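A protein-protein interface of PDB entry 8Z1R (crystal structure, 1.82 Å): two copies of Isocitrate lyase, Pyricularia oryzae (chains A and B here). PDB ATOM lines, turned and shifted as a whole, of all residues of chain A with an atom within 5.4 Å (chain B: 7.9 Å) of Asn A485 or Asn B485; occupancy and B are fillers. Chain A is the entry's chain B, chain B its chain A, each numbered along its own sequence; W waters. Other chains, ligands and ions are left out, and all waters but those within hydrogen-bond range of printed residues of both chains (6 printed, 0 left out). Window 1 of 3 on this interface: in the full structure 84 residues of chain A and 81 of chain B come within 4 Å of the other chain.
OD1 of Asn B485 lies within hydrogen-bond range of NE2 of Gln A102, 2.9 Å away.
The side-chain carboxylate of Asp B99 is in hydrogen-bond range of the side-chain amide nitrogen of Asn A485 (2.6 Å).
The side-chain carboxylate (OD2) of Asp A99 sits at hydrogen-bond distance from the side-chain amide nitrogen (ND2) of Asn B485 (2.7 Å).
The side-chain amide oxygen (OD1) of Asn A485 sits close to the side-chain amide oxygen (OD1) of Asn B485, 3.4 Å away.
The side-chain sulfur of Cys A490 sits close to the side-chain amide oxygen of Gln B105.
ND1 of His A483 lies within hydrogen-bond range of OE2 of Glu B512.
The side-chain amide oxygen of Asn A485 is in hydrogen-bond range of the side-chain amide nitrogen of Gln B102, 2.9 Å away.
The backbone carbonyl oxygen of Glu B512 sits at hydrogen-bond distance from the backbone NH of Cys B517 (3.1 Å).
OG1 of Thr A489 sits at hydrogen-bond distance from O of Asn A485 (3.4 Å).
The side-chain carboxylate (OD1) of Asp B99 is in hydrogen-bond range of the backbone NH (N) of Gln B102.
The side-chain carboxylate (OD1) of Asp B99 sits at hydrogen-bond distance from the backbone NH (N) of Ile B101 (2.9 Å).
OD1 of Asp A99 is in hydrogen-bond range of N of Ile A101, at 2.8 Å.
Among the printed residues, merely in contact across the chains: Thr A487 with Glu B512, Gln A102 with Thr B489, Thr A489 with Gln B102, His A483 with Val B519, Ala A486 with Val B519, Ala A486 with Ile B101, Ala A486 with Gln B105, Ile A101 with Val B123, Ile A101 with Ala B486, His A483 with Val B508, Val A482 with Ile B101, Thr A484 with Val B508, Ile A101 with Val B482, Thr A484 with Ala B488, Ile A98 with Ile B101, Ile A101 with Ile B98, Thr A489 with Gln B105, Ala A486 with Cys B517, Ala A488 with Thr B484, Thr A489 with Thr B484, Thr A484 with Thr B489, Ile A101 with Asn B485, Cys A490 with Cys B517, Val A482 with Val B519 and Ala A488 with Ala B488.
Asn A485 touches just these residues of chain B: Asp B99, Gln B102 and Asn B485.
Of the printed residues of chain B, Thr A487 touches Glu B512.
Printed residues of chain A within 4 Å of Val B123: Ile A101.
Ala B480 touches none of the printed residues of chain A.
Asn B485 touches four residues of chain A.
Of the printed residues of chain A, Ala B486 touches Ile A101.
Glu B491 touches none of the printed residues of chain A.
The nearest residue of chain B that does not touch Asn A485 is Ile B101 (4.05 Å).
The nearest residue of chain A that does not touch Asn B485 is Gly A481 (4.9 Å).
The nearest printed residue of chain B that does not touch Ile A101 is Gly B481 (5.1 Å).
Of the 15 printed residues of chain A, 13 touch a printed residue of chain B.
Among the printed residues, 32 pairs touch across the chains.
Among the printed residues, no Asp or Glu carboxylate lies within 4 Å of a Lys or Arg side-chain nitrogen of the other chain.
Ile A98 touches Ile B101, and with the chains exchanged Ile A101 touches Ile B98.
Ile A101 touches Asn B485, but with the chains exchanged Asn A485 does not touch Ile B101 (4.05 Å).
Gln A102 touches Asn B485, and with the chains exchanged Asn A485 touches Gln B102.
Thr A484 touches Ala B488, and with the chains exchanged Ala A488 touches Thr B484.
Water W4 lies within hydrogen-bond range of the side-chain hydroxyl (OG1) of Thr A484 (2.7 Å) and the side-chain hydroxyl (OG1) of Thr B489 (2.9 Å).
Water W2 bridges the side-chain carboxylate of Asp A99 (2.7 Å) and the side-chain carboxylate of Asp B99 (2.7 Å).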
ATOM      1  N   ILE A  98     -18.835  11.408 -24.674  1.00  0.00           N
ATOM      2  CA  ILE A  98     -18.051  12.218 -23.748  1.00  0.00           C
ATOM      3  C   ILE A  98     -18.889  12.820 -22.633  1.00  0.00           C
ATOM      4  O   ILE A  98     -18.329  13.491 -21.749  1.00  0.00           O
ATOM      5  CB  ILE A  98     -17.266  13.328 -24.479  1.00  0.00           C
ATOM      6  CG1 ILE A  98     -18.213  14.340 -25.100  1.00  0.00           C
ATOM      7  CG2 ILE A  98     -16.364  12.725 -25.579  1.00  0.00           C
ATOM      8  CD1 ILE A  98     -17.515  15.661 -25.498  1.00  0.00           C
ATOM      9  N   ASP A  99     -20.196  12.591 -22.622  1.00  0.00           N
ATOM     10  CA  ASP A  99     -21.036  13.203 -21.600  1.00  0.00           C
ATOM     11  C   ASP A  99     -22.369  12.464 -21.549  1.00  0.00           C
ATOM     12  O   ASP A  99     -22.692  11.679 -22.457  1.00  0.00           O
ATOM     13  CB  ASP A  99     -21.237  14.706 -21.874  1.00  0.00           C
ATOM     14  CG  ASP A  99     -21.924  14.972 -23.189  1.00  0.00           C
ATOM     15  OD1 ASP A  99     -23.046  14.453 -23.396  1.00  0.00           O
ATOM     16  OD2 ASP A  99     -21.354  15.727 -24.008  1.00  0.00           O
ATOM     17  N   ILE A 101     -25.348  13.576 -22.125  1.00  0.00           N
ATOM     18  CA  ILE A 101     -26.244  13.902 -23.233  1.00  0.00           C
ATOM     19  C   ILE A 101     -26.029  12.934 -24.383  1.00  0.00           C
ATOM     20  O   ILE A 101     -26.983  12.387 -24.950  1.00  0.00           O
ATOM     21  CB  ILE A 101     -26.041  15.357 -23.683  1.00  0.00           C
ATOM     22  CG1 ILE A 101     -26.481  16.317 -22.572  1.00  0.00           C
ATOM     23  CG2 ILE A 101     -26.833  15.634 -24.938  1.00  0.00           C
ATOM     24  CD1 ILE A 101     -25.947  17.708 -22.777  1.00  0.00           C
ATOM     25  N   GLN A 102     -24.771  12.724 -24.765  1.00  0.00           N
ATOM     26  CA  GLN A 102     -24.525  11.809 -25.869  1.00  0.00           C
ATOM     27  C   GLN A 102     -24.985  10.399 -25.518  1.00  0.00           C
ATOM     28  O   GLN A 102     -25.557   9.705 -26.372  1.00  0.00           O
ATOM     29  CB  GLN A 102     -23.042  11.848 -26.252  1.00  0.00           C
ATOM     30  CG  GLN A 102     -22.643  13.248 -26.750  1.00  0.00           C
ATOM     31  CD  GLN A 102     -21.209  13.325 -27.202  1.00  0.00           C
ATOM     32  OE1 GLN A 102     -20.442  12.387 -26.997  1.00  0.00           O
ATOM     33  NE2 GLN A 102     -20.835  14.446 -27.827  1.00  0.00           N
ATOM     34  N   ALA A 480     -15.754   9.885 -31.649  1.00  0.00           N
ATOM     35  CA  ALA A 480     -16.935  10.361 -32.370  1.00  0.00           C
ATOM     36  C   ALA A 480     -17.577  11.551 -31.666  1.00  0.00           C
ATOM     37  O   ALA A 480     -17.893  12.561 -32.303  1.00  0.00           O
ATOM     38  CB  ALA A 480     -17.968   9.240 -32.511  1.00  0.00           C
ATOM     39  N   GLY A 481     -17.772  11.449 -30.351  1.00  0.00           N
ATOM     40  CA  GLY A 481     -18.447  12.505 -29.616  1.00  0.00           C
ATOM     41  C   GLY A 481     -17.643  13.784 -29.487  1.00  0.00           C
ATOM     42  O   GLY A 481     -18.228  14.853 -29.261  1.00  0.00           O
ATOM     43  N   VAL A 482     -16.319  13.703 -29.620  1.00  0.00           N
ATOM     44  CA  VAL A 482     -15.519  14.921 -29.721  1.00  0.00           C
ATOM     45  C   VAL A 482     -15.846  15.665 -31.015  1.00  0.00           C
ATOM     46  O   VAL A 482     -16.062  16.885 -31.017  1.00  0.00           O
ATOM     47  CB  VAL A 482     -14.018  14.581 -29.620  1.00  0.00           C
ATOM     48  CG1 VAL A 482     -13.162  15.832 -29.823  1.00  0.00           C
ATOM     49  CG2 VAL A 482     -13.711  13.985 -28.262  1.00  0.00           C
ATOM     50  N   HIS A 483     -15.898  14.936 -32.136  1.00  0.00           N
ATOM     51  CA  HIS A 483     -16.021  15.569 -33.443  1.00  0.00           C
ATOM     52  C   HIS A 483     -17.430  16.114 -33.696  1.00  0.00           C
ATOM     53  O   HIS A 483     -17.580  17.204 -34.261  1.00  0.00           O
ATOM     54  CB  HIS A 483     -15.600  14.579 -34.545  1.00  0.00           C
ATOM     55  CG  HIS A 483     -14.121  14.315 -34.582  1.00  0.00           C
ATOM     56  ND1 HIS A 483     -13.206  15.273 -34.965  1.00  0.00           N
ATOM     57  CD2 HIS A 483     -13.398  13.211 -34.273  1.00  0.00           C
ATOM     58  CE1 HIS A 483     -11.982  14.767 -34.899  1.00  0.00           C
ATOM     59  NE2 HIS A 483     -12.072  13.515 -34.489  1.00  0.00           N
ATOM     60  N   THR A 484     -18.478  15.376 -33.314  1.00  0.00           N
ATOM     61  CA  THR A 484     -19.823  15.904 -33.532  1.00  0.00           C
ATOM     62  C   THR A 484     -20.043  17.161 -32.708  1.00  0.00           C
ATOM     63  O   THR A 484     -20.686  18.108 -33.166  1.00  0.00           O
ATOM     64  CB  THR A 484     -20.897  14.872 -33.174  1.00  0.00           C
ATOM     65  OG1 THR A 484     -20.722  14.463 -31.809  1.00  0.00           O
ATOM     66  CG2 THR A 484     -20.820  13.659 -34.090  1.00  0.00           C
ATOM     67  N   ASN A 485     -19.530  17.167 -31.480  1.00  0.00           N
ATOM     68  CA  ASN A 485     -19.704  18.313 -30.592  1.00  0.00           C
ATOM     69  C   ASN A 485     -18.971  19.532 -31.143  1.00  0.00           C
ATOM     70  O   ASN A 485     -19.540  20.627 -31.243  1.00  0.00           O
ATOM     71  CB  ASN A 485     -19.202  17.928 -29.195  1.00  0.00           C
ATOM     72  CG  ASN A 485     -19.640  18.890 -28.111  1.00  0.00           C
ATOM     73  OD1 ASN A 485     -20.643  19.599 -28.241  1.00  0.00           O
ATOM     74  ND2 ASN A 485     -18.889  18.902 -27.014  1.00  0.00           N
ATOM     75  N   ALA A 486     -17.718  19.344 -31.556  1.00  0.00           N
ATOM     76  CA  ALA A 486     -16.927  20.447 -32.101  1.00  0.00           C
ATOM     77  C   ALA A 486     -17.567  21.033 -33.357  1.00  0.00           C
ATOM     78  O   ALA A 486     -17.608  22.257 -33.542  1.00  0.00           O
ATOM     79  CB  ALA A 486     -15.511  19.960 -32.415  1.00  0.00           C
ATOM     80  N   THR A 487     -18.027  20.164 -34.252  1.00  0.00           N
ATOM     81  CA  THR A 487     -18.578  20.619 -35.515  1.00  0.00           C
ATOM     82  C   THR A 487     -19.848  21.424 -35.278  1.00  0.00           C
ATOM     83  O   THR A 487     -20.031  22.506 -35.844  1.00  0.00           O
ATOM     84  CB  THR A 487     -18.845  19.409 -36.420  1.00  0.00           C
ATOM     85  OG1 THR A 487     -17.606  18.732 -36.686  1.00  0.00           O
ATOM     86  CG2 THR A 487     -19.508  19.837 -37.728  1.00  0.00           C
ATOM     87  N   ALA A 488     -20.729  20.913 -34.420  1.00  0.00           N
ATOM     88  CA  ALA A 488     -21.997  21.597 -34.188  1.00  0.00           C
ATOM     89  C   ALA A 488     -21.783  22.969 -33.558  1.00  0.00           C
ATOM     90  O   ALA A 488     -22.474  23.935 -33.916  1.00  0.00           O
ATOM     91  CB  ALA A 488     -22.907  20.735 -33.312  1.00  0.00           C
ATOM     92  N   THR A 489     -20.840  23.082 -32.616  1.00  0.00           N
ATOM     93  CA  THR A 489     -20.626  24.394 -32.006  1.00  0.00           C
ATOM     94  C   THR A 489     -19.897  25.336 -32.957  1.00  0.00           C
ATOM     95  O   THR A 489     -20.184  26.541 -32.987  1.00  0.00           O
ATOM     96  CB  THR A 489     -19.861  24.266 -30.686  1.00  0.00           C
ATOM     97  OG1 THR A 489     -20.609  23.463 -29.758  1.00  0.00           O
ATOM     98  CG2 THR A 489     -19.636  25.667 -30.066  1.00  0.00           C
ATOM     99  N   CYS A 490     -18.959  24.808 -33.745  1.00  0.00           N
ATOM    100  CA  CYS A 490     -18.267  25.635 -34.730  1.00  0.00           C
ATOM    101  C   CYS A 490     -19.265  26.323 -35.660  1.00  0.00           C
ATOM    102  O   CYS A 490     -19.201  27.540 -35.886  1.00  0.00           O
ATOM    103  CB  CYS A 490     -17.286  24.766 -35.519  1.00  0.00           C
ATOM    104  SG  CYS A 490     -16.342  25.651 -36.787  1.00  0.00           S
ATOM    105  N   ILE B  98     -20.752  23.837 -22.287  1.00  0.00           N
ATOM    106  CA  ILE B  98     -20.782  22.788 -21.278  1.00  0.00           C
ATOM    107  C   ILE B  98     -19.478  22.025 -21.188  1.00  0.00           C
ATOM    108  O   ILE B  98     -19.359  21.149 -20.323  1.00  0.00           O
ATOM    109  CB  ILE B  98     -21.955  21.816 -21.508  1.00  0.00           C
ATOM    110  CG1 ILE B  98     -21.729  20.971 -22.761  1.00  0.00           C
ATOM    111  CG2 ILE B  98     -23.271  22.599 -21.642  1.00  0.00           C
ATOM    112  CD1 ILE B  98     -22.799  19.899 -22.983  1.00  0.00           C
ATOM    113  N   ASP B  99     -18.496  22.324 -22.032  1.00  0.00           N
ATOM    114  CA  ASP B  99     -17.259  21.553 -22.029  1.00  0.00           C
ATOM    115  C   ASP B  99     -16.170  22.359 -22.738  1.00  0.00           C
ATOM    116  O   ASP B  99     -16.460  23.361 -23.408  1.00  0.00           O
ATOM    117  CB  ASP B  99     -17.465  20.176 -22.687  1.00  0.00           C
ATOM    118  CG  ASP B  99     -17.854  20.272 -24.149  1.00  0.00           C
ATOM    119  OD1 ASP B  99     -17.133  20.951 -24.916  1.00  0.00           O
ATOM    120  OD2 ASP B  99     -18.866  19.632 -24.534  1.00  0.00           O
ATOM    121  N   PRO B 100     -14.903  21.947 -22.601  1.00  0.00           N
ATOM    122  CA  PRO B 100     -13.801  22.697 -23.236  1.00  0.00           C
ATOM    123  C   PRO B 100     -13.833  22.711 -24.753  1.00  0.00           C
ATOM    124  O   PRO B 100     -13.317  23.665 -25.345  1.00  0.00           O
ATOM    125  CB  PRO B 100     -12.547  21.976 -22.722  1.00  0.00           C
ATOM    126  CG  PRO B 100     -12.954  21.424 -21.399  1.00  0.00           C
ATOM    127  CD  PRO B 100     -14.416  21.053 -21.536  1.00  0.00           C
ATOM    128  N   ILE B 101     -14.384  21.680 -25.401  1.00  0.00           N
ATOM    129  CA  ILE B 101     -14.525  21.692 -26.858  1.00  0.00           C
ATOM    130  C   ILE B 101     -15.378  22.873 -27.305  1.00  0.00           C
ATOM    131  O   ILE B 101     -15.041  23.584 -28.262  1.00  0.00           O
ATOM    132  CB  ILE B 101     -15.131  20.365 -27.351  1.00  0.00           C
ATOM    133  CG1 ILE B 101     -14.229  19.179 -26.993  1.00  0.00           C
ATOM    134  CG2 ILE B 101     -15.378  20.424 -28.855  1.00  0.00           C
ATOM    135  CD1 ILE B 101     -14.907  17.838 -27.223  1.00  0.00           C
ATOM    136  N   GLN B 102     -16.533  23.065 -26.652  1.00  0.00           N
ATOM    137  CA  GLN B 102     -17.396  24.179 -27.022  1.00  0.00           C
ATOM    138  C   GLN B 102     -16.703  25.516 -26.773  1.00  0.00           C
ATOM    139  O   GLN B 102     -16.799  26.434 -27.603  1.00  0.00           O
ATOM    140  CB  GLN B 102     -18.724  24.083 -26.265  1.00  0.00           C
ATOM    141  CG  GLN B 102     -19.495  22.817 -26.667  1.00  0.00           C
ATOM    142  CD  GLN B 102     -20.873  22.722 -26.055  1.00  0.00           C
ATOM    143  OE1 GLN B 102     -21.225  23.494 -25.166  1.00  0.00           O
ATOM    144  NE2 GLN B 102     -21.674  21.770 -26.543  1.00  0.00           N
ATOM    145  N   MET B 103     -15.965  25.630 -25.665  1.00  0.00           N
ATOM    146  CA  MET B 103     -15.185  26.844 -25.424  1.00  0.00           C
ATOM    147  C   MET B 103     -14.231  27.127 -26.585  1.00  0.00           C
ATOM    148  O   MET B 103     -14.139  28.265 -27.066  1.00  0.00           O
ATOM    149  CB  MET B 103     -14.414  26.727 -24.105  1.00  0.00           C
ATOM    150  CG  MET B 103     -13.482  27.923 -23.774  1.00  0.00           C
ATOM    151  SD  MET B 103     -11.852  27.851 -24.568  1.00  0.00           S
ATOM    152  CE  MET B 103     -11.196  26.372 -23.774  1.00  0.00           C
ATOM    153  N   GLN B 105     -14.369  26.305 -29.659  1.00  0.00           N
ATOM    154  CA  GLN B 105     -15.034  26.655 -30.910  1.00  0.00           C
ATOM    155  C   GLN B 105     -15.764  27.995 -30.845  1.00  0.00           C
ATOM    156  O   GLN B 105     -16.081  28.551 -31.901  1.00  0.00           O
ATOM    157  CB  GLN B 105     -16.007  25.544 -31.325  1.00  0.00           C
ATOM    158  CG  GLN B 105     -15.302  24.216 -31.575  1.00  0.00           C
ATOM    159  CD  GLN B 105     -14.177  24.357 -32.573  1.00  0.00           C
ATOM    160  OE1 GLN B 105     -14.413  24.714 -33.713  1.00  0.00           O
ATOM    161  NE2 GLN B 105     -12.949  24.121 -32.135  1.00  0.00           N
ATOM    162  N   VAL B 123     -25.437  17.237 -16.492  1.00  0.00           N
ATOM    163  CA  VAL B 123     -24.285  16.739 -17.252  1.00  0.00           C
ATOM    164  C   VAL B 123     -22.982  16.655 -16.442  1.00  0.00           C
ATOM    165  O   VAL B 123     -22.086  15.877 -16.805  1.00  0.00           O
ATOM    166  CB  VAL B 123     -24.043  17.572 -18.536  1.00  0.00           C
ATOM    167  CG1 VAL B 123     -25.358  17.977 -19.215  1.00  0.00           C
ATOM    168  CG2 VAL B 123     -23.167  18.779 -18.280  1.00  0.00           C
ATOM    169  N   ARG B 148     -12.891  23.802 -14.735  1.00  0.00           N
ATOM    170  CA  ARG B 148     -12.619  22.938 -15.881  1.00  0.00           C
ATOM    171  C   ARG B 148     -12.473  23.766 -17.155  1.00  0.00           C
ATOM    172  O   ARG B 148     -11.554  23.547 -17.955  1.00  0.00           O
ATOM    173  CB  ARG B 148     -13.746  21.914 -16.002  1.00  0.00           C
ATOM    174  CG  ARG B 148     -13.797  21.134 -17.293  1.00  0.00           C
ATOM    175  CD  ARG B 148     -15.060  20.282 -17.329  1.00  0.00           C
ATOM    176  NE  ARG B 148     -15.115  19.390 -18.482  1.00  0.00           N
ATOM    177  CZ  ARG B 148     -16.237  18.968 -19.051  1.00  0.00           C
ATOM    178  NH1 ARG B 148     -17.424  19.418 -18.664  1.00  0.00           N
ATOM    179  NH2 ARG B 148     -16.169  18.092 -20.047  1.00  0.00           N
ATOM    180  N   LEU B 479     -28.926  27.287 -22.524  1.00  0.00           N
ATOM    181  CA  LEU B 479     -28.736  25.861 -22.770  1.00  0.00           C
ATOM    182  C   LEU B 479     -28.225  25.551 -24.182  1.00  0.00           C
ATOM    183  O   LEU B 479     -28.387  24.420 -24.655  1.00  0.00           O
ATOM    184  CB  LEU B 479     -30.040  25.109 -22.503  1.00  0.00           C
ATOM    185  CG  LEU B 479     -30.548  25.097 -21.055  1.00  0.00           C
ATOM    186  CD1 LEU B 479     -31.688  24.093 -20.916  1.00  0.00           C
ATOM    187  CD2 LEU B 479     -29.427  24.799 -20.052  1.00  0.00           C
ATOM    188  N   ALA B 480     -27.608  26.520 -24.862  1.00  0.00           N
ATOM    189  CA  ALA B 480     -27.259  26.326 -26.269  1.00  0.00           C
ATOM    190  C   ALA B 480     -26.401  25.074 -26.464  1.00  0.00           C
ATOM    191  O   ALA B 480     -26.673  24.252 -27.346  1.00  0.00           O
ATOM    192  CB  ALA B 480     -26.525  27.559 -26.802  1.00  0.00           C
ATOM    193  N   GLY B 481     -25.382  24.900 -25.619  1.00  0.00           N
ATOM    194  CA  GLY B 481     -24.455  23.782 -25.775  1.00  0.00           C
ATOM    195  C   GLY B 481     -25.057  22.424 -25.461  1.00  0.00           C
ATOM    196  O   GLY B 481     -24.561  21.410 -25.960  1.00  0.00           O
ATOM    197  N   VAL B 482     -26.096  22.382 -24.626  1.00  0.00           N
ATOM    198  CA  VAL B 482     -26.860  21.153 -24.437  1.00  0.00           C
ATOM    199  C   VAL B 482     -27.563  20.768 -25.731  1.00  0.00           C
ATOM    200  O   VAL B 482     -27.511  19.613 -26.173  1.00  0.00           O
ATOM    201  CB  VAL B 482     -27.879  21.328 -23.293  1.00  0.00           C
ATOM    202  CG1 VAL B 482     -28.822  20.133 -23.235  1.00  0.00           C
ATOM    203  CG2 VAL B 482     -27.177  21.543 -21.963  1.00  0.00           C
ATOM    204  N   HIS B 483     -28.245  21.734 -26.352  1.00  0.00           N
ATOM    205  CA  HIS B 483     -29.087  21.428 -27.507  1.00  0.00           C
ATOM    206  C   HIS B 483     -28.268  21.105 -28.757  1.00  0.00           C
ATOM    207  O   HIS B 483     -28.643  20.204 -29.521  1.00  0.00           O
ATOM    208  CB  HIS B 483     -30.050  22.586 -27.773  1.00  0.00           C
ATOM    209  CG  HIS B 483     -31.135  22.703 -26.750  1.00  0.00           C
ATOM    210  ND1 HIS B 483     -32.162  21.790 -26.649  1.00  0.00           N
ATOM    211  CD2 HIS B 483     -31.354  23.620 -25.778  1.00  0.00           C
ATOM    212  CE1 HIS B 483     -32.972  22.144 -25.665  1.00  0.00           C
ATOM    213  NE2 HIS B 483     -32.499  23.247 -25.116  1.00  0.00           N
ATOM    214  N   THR B 484     -27.170  21.838 -29.010  1.00  0.00           N
ATOM    215  CA  THR B 484     -26.355  21.518 -30.185  1.00  0.00           C
ATOM    216  C   THR B 484     -25.782  20.119 -30.070  1.00  0.00           C
ATOM    217  O   THR B 484     -25.750  19.366 -31.052  1.00  0.00           O
ATOM    218  CB  THR B 484     -25.210  22.519 -30.387  1.00  0.00           C
ATOM    219  OG1 THR B 484     -24.347  22.539 -29.236  1.00  0.00           O
ATOM    220  CG2 THR B 484     -25.760  23.933 -30.660  1.00  0.00           C
ATOM    221  N   ASN B 485     -25.312  19.766 -28.872  1.00  0.00           N
ATOM    222  CA  ASN B 485     -24.695  18.466 -28.622  1.00  0.00           C
ATOM    223  C   ASN B 485     -25.721  17.349 -28.767  1.00  0.00           C
ATOM    224  O   ASN B 485     -25.470  16.344 -29.442  1.00  0.00           O
ATOM    225  CB  ASN B 485     -24.068  18.510 -27.223  1.00  0.00           C
ATOM    226  CG  ASN B 485     -23.149  17.345 -26.923  1.00  0.00           C
ATOM    227  OD1 ASN B 485     -22.490  16.801 -27.807  1.00  0.00           O
ATOM    228  ND2 ASN B 485     -23.080  16.977 -25.644  1.00  0.00           N
ATOM    229  N   ALA B 486     -26.910  17.529 -28.182  1.00  0.00           N
ATOM    230  CA  ALA B 486     -27.949  16.507 -28.298  1.00  0.00           C
ATOM    231  C   ALA B 486     -28.346  16.273 -29.751  1.00  0.00           C
ATOM    232  O   ALA B 486     -28.512  15.126 -30.183  1.00  0.00           O
ATOM    233  CB  ALA B 486     -29.179  16.921 -27.485  1.00  0.00           C
ATOM    234  N   THR B 487     -28.523  17.355 -30.513  1.00  0.00           N
ATOM    235  CA  THR B 487     -29.006  17.235 -31.883  1.00  0.00           C
ATOM    236  C   THR B 487     -27.972  16.547 -32.768  1.00  0.00           C
ATOM    237  O   THR B 487     -28.314  15.698 -33.599  1.00  0.00           O
ATOM    238  CB  THR B 487     -29.360  18.626 -32.420  1.00  0.00           C
ATOM    239  OG1 THR B 487     -30.378  19.203 -31.592  1.00  0.00           O
ATOM    240  CG2 THR B 487     -29.858  18.562 -33.869  1.00  0.00           C
ATOM    241  N   ALA B 488     -26.699  16.902 -32.602  1.00  0.00           N
ATOM    242  CA  ALA B 488     -25.656  16.309 -33.435  1.00  0.00           C
ATOM    243  C   ALA B 488     -25.538  14.807 -33.182  1.00  0.00           C
ATOM    244  O   ALA B 488     -25.410  14.010 -34.124  1.00  0.00           O
ATOM    245  CB  ALA B 488     -24.324  17.009 -33.167  1.00  0.00           C
ATOM    246  N   THR B 489     -25.592  14.399 -31.910  1.00  0.00           N
ATOM    247  CA  THR B 489     -25.464  12.979 -31.582  1.00  0.00           C
ATOM    248  C   THR B 489     -26.713  12.203 -31.997  1.00  0.00           C
ATOM    249  O   THR B 489     -26.607  11.089 -32.528  1.00  0.00           O
ATOM    250  CB  THR B 489     -25.156  12.815 -30.089  1.00  0.00           C
ATOM    251  OG1 THR B 489     -23.889  13.425 -29.805  1.00  0.00           O
ATOM    252  CG2 THR B 489     -25.083  11.338 -29.690  1.00  0.00           C
ATOM    253  N   CYS B 490     -27.898  12.792 -31.810  1.00  0.00           N
ATOM    254  CA  CYS B 490     -29.136  12.155 -32.258  1.00  0.00           C
ATOM    255  C   CYS B 490     -29.082  11.816 -33.749  1.00  0.00           C
ATOM    256  O   CYS B 490     -29.375  10.682 -34.158  1.00  0.00           O
ATOM    257  CB  CYS B 490     -30.322  13.074 -31.953  1.00  0.00           C
ATOM    258  SG  CYS B 490     -31.920  12.382 -32.500  1.00  0.00           S
ATOM    259  N   GLU B 491     -28.679  12.787 -34.574  1.00  0.00           N
ATOM    260  CA  GLU B 491     -28.593  12.568 -36.015  1.00  0.00           C
ATOM    261  C   GLU B 491     -27.597  11.461 -36.346  1.00  0.00           C
ATOM    262  O   GLU B 491     -27.900  10.542 -37.114  1.00  0.00           O
ATOM    263  CB  GLU B 491     -28.195  13.873 -36.697  1.00  0.00           C
ATOM    264  CG  GLU B 491     -28.228  13.845 -38.208  1.00  0.00           C
ATOM    265  CD  GLU B 491     -27.729  15.144 -38.819  1.00  0.00           C
ATOM    266  OE1 GLU B 491     -26.640  15.625 -38.425  1.00  0.00           O
ATOM    267  OE2 GLU B 491     -28.427  15.682 -39.697  1.00  0.00           O
ATOM    268  N   VAL B 508     -20.254  13.763 -40.360  1.00  0.00           N
ATOM    269  CA  VAL B 508     -19.277  14.342 -39.452  1.00  0.00           C
ATOM    270  C   VAL B 508     -18.034  14.758 -40.225  1.00  0.00           C
ATOM    271  O   VAL B 508     -17.771  15.953 -40.387  1.00  0.00           O
ATOM    272  CB  VAL B 508     -18.929  13.372 -38.303  1.00  0.00           C
ATOM    273  CG1 VAL B 508     -18.091  14.082 -37.251  1.00  0.00           C
ATOM    274  CG2 VAL B 508     -20.200  12.828 -37.668  1.00  0.00           C
ATOM    275  N   GLU B 512     -17.209  18.566 -41.051  1.00  0.00           N
ATOM    276  CA  GLU B 512     -16.127  19.165 -40.279  1.00  0.00           C
ATOM    277  C   GLU B 512     -15.083  19.782 -41.202  1.00  0.00           C
ATOM    278  O   GLU B 512     -14.605  20.899 -40.961  1.00  0.00           O
ATOM    279  CB  GLU B 512     -15.505  18.094 -39.379  1.00  0.00           C
ATOM    280  CG  GLU B 512     -14.716  18.581 -38.189  1.00  0.00           C
ATOM    281  CD  GLU B 512     -14.252  17.416 -37.315  1.00  0.00           C
ATOM    282  OE1 GLU B 512     -14.453  16.248 -37.720  1.00  0.00           O
ATOM    283  OE2 GLU B 512     -13.690  17.665 -36.230  1.00  0.00           O
ATOM    284  N   CYS B 517     -13.553  23.314 -39.313  1.00  0.00           N
ATOM    285  CA  CYS B 517     -13.455  23.141 -37.867  1.00  0.00           C
ATOM    286  C   CYS B 517     -12.072  22.596 -37.505  1.00  0.00           C
ATOM    287  O   CYS B 517     -11.675  21.528 -37.980  1.00  0.00           O
ATOM    288  CB  CYS B 517     -14.556  22.200 -37.385  1.00  0.00           C
ATOM    289  SG  CYS B 517     -14.402  21.712 -35.655  1.00  0.00           S
ATOM    290  N   VAL B 519     -10.881  21.111 -35.048  1.00  0.00           N
ATOM    291  CA  VAL B 519     -10.770  19.846 -34.321  1.00  0.00           C
ATOM    292  C   VAL B 519     -10.543  18.674 -35.275  1.00  0.00           C
ATOM    293  O   VAL B 519     -10.147  17.585 -34.835  1.00  0.00           O
ATOM    294  CB  VAL B 519     -12.022  19.646 -33.446  1.00  0.00           C
ATOM    295  CG1 VAL B 519     -11.955  18.325 -32.639  1.00  0.00           C
ATOM    296  CG2 VAL B 519     -12.174  20.833 -32.503  1.00  0.00           C
HETATM  297  O   HOH W   1     -22.276  21.132 -29.682  1.00  0.00           O
HETATM  298  O   HOH W   2     -19.569  17.485 -23.010  1.00  0.00           O
HETATM  299  O   HOH W   3     -22.908  24.908 -29.061  1.00  0.00           O
HETATM  300  O   HOH W   4     -21.801  12.091 -31.233  1.00  0.00           O
HETATM  301  O   HOH W   5     -22.505  15.707 -30.411  1.00  0.00           O
HETATM  302  O   HOH W   6     -17.717  16.330 -21.538  1.00  0.00           O
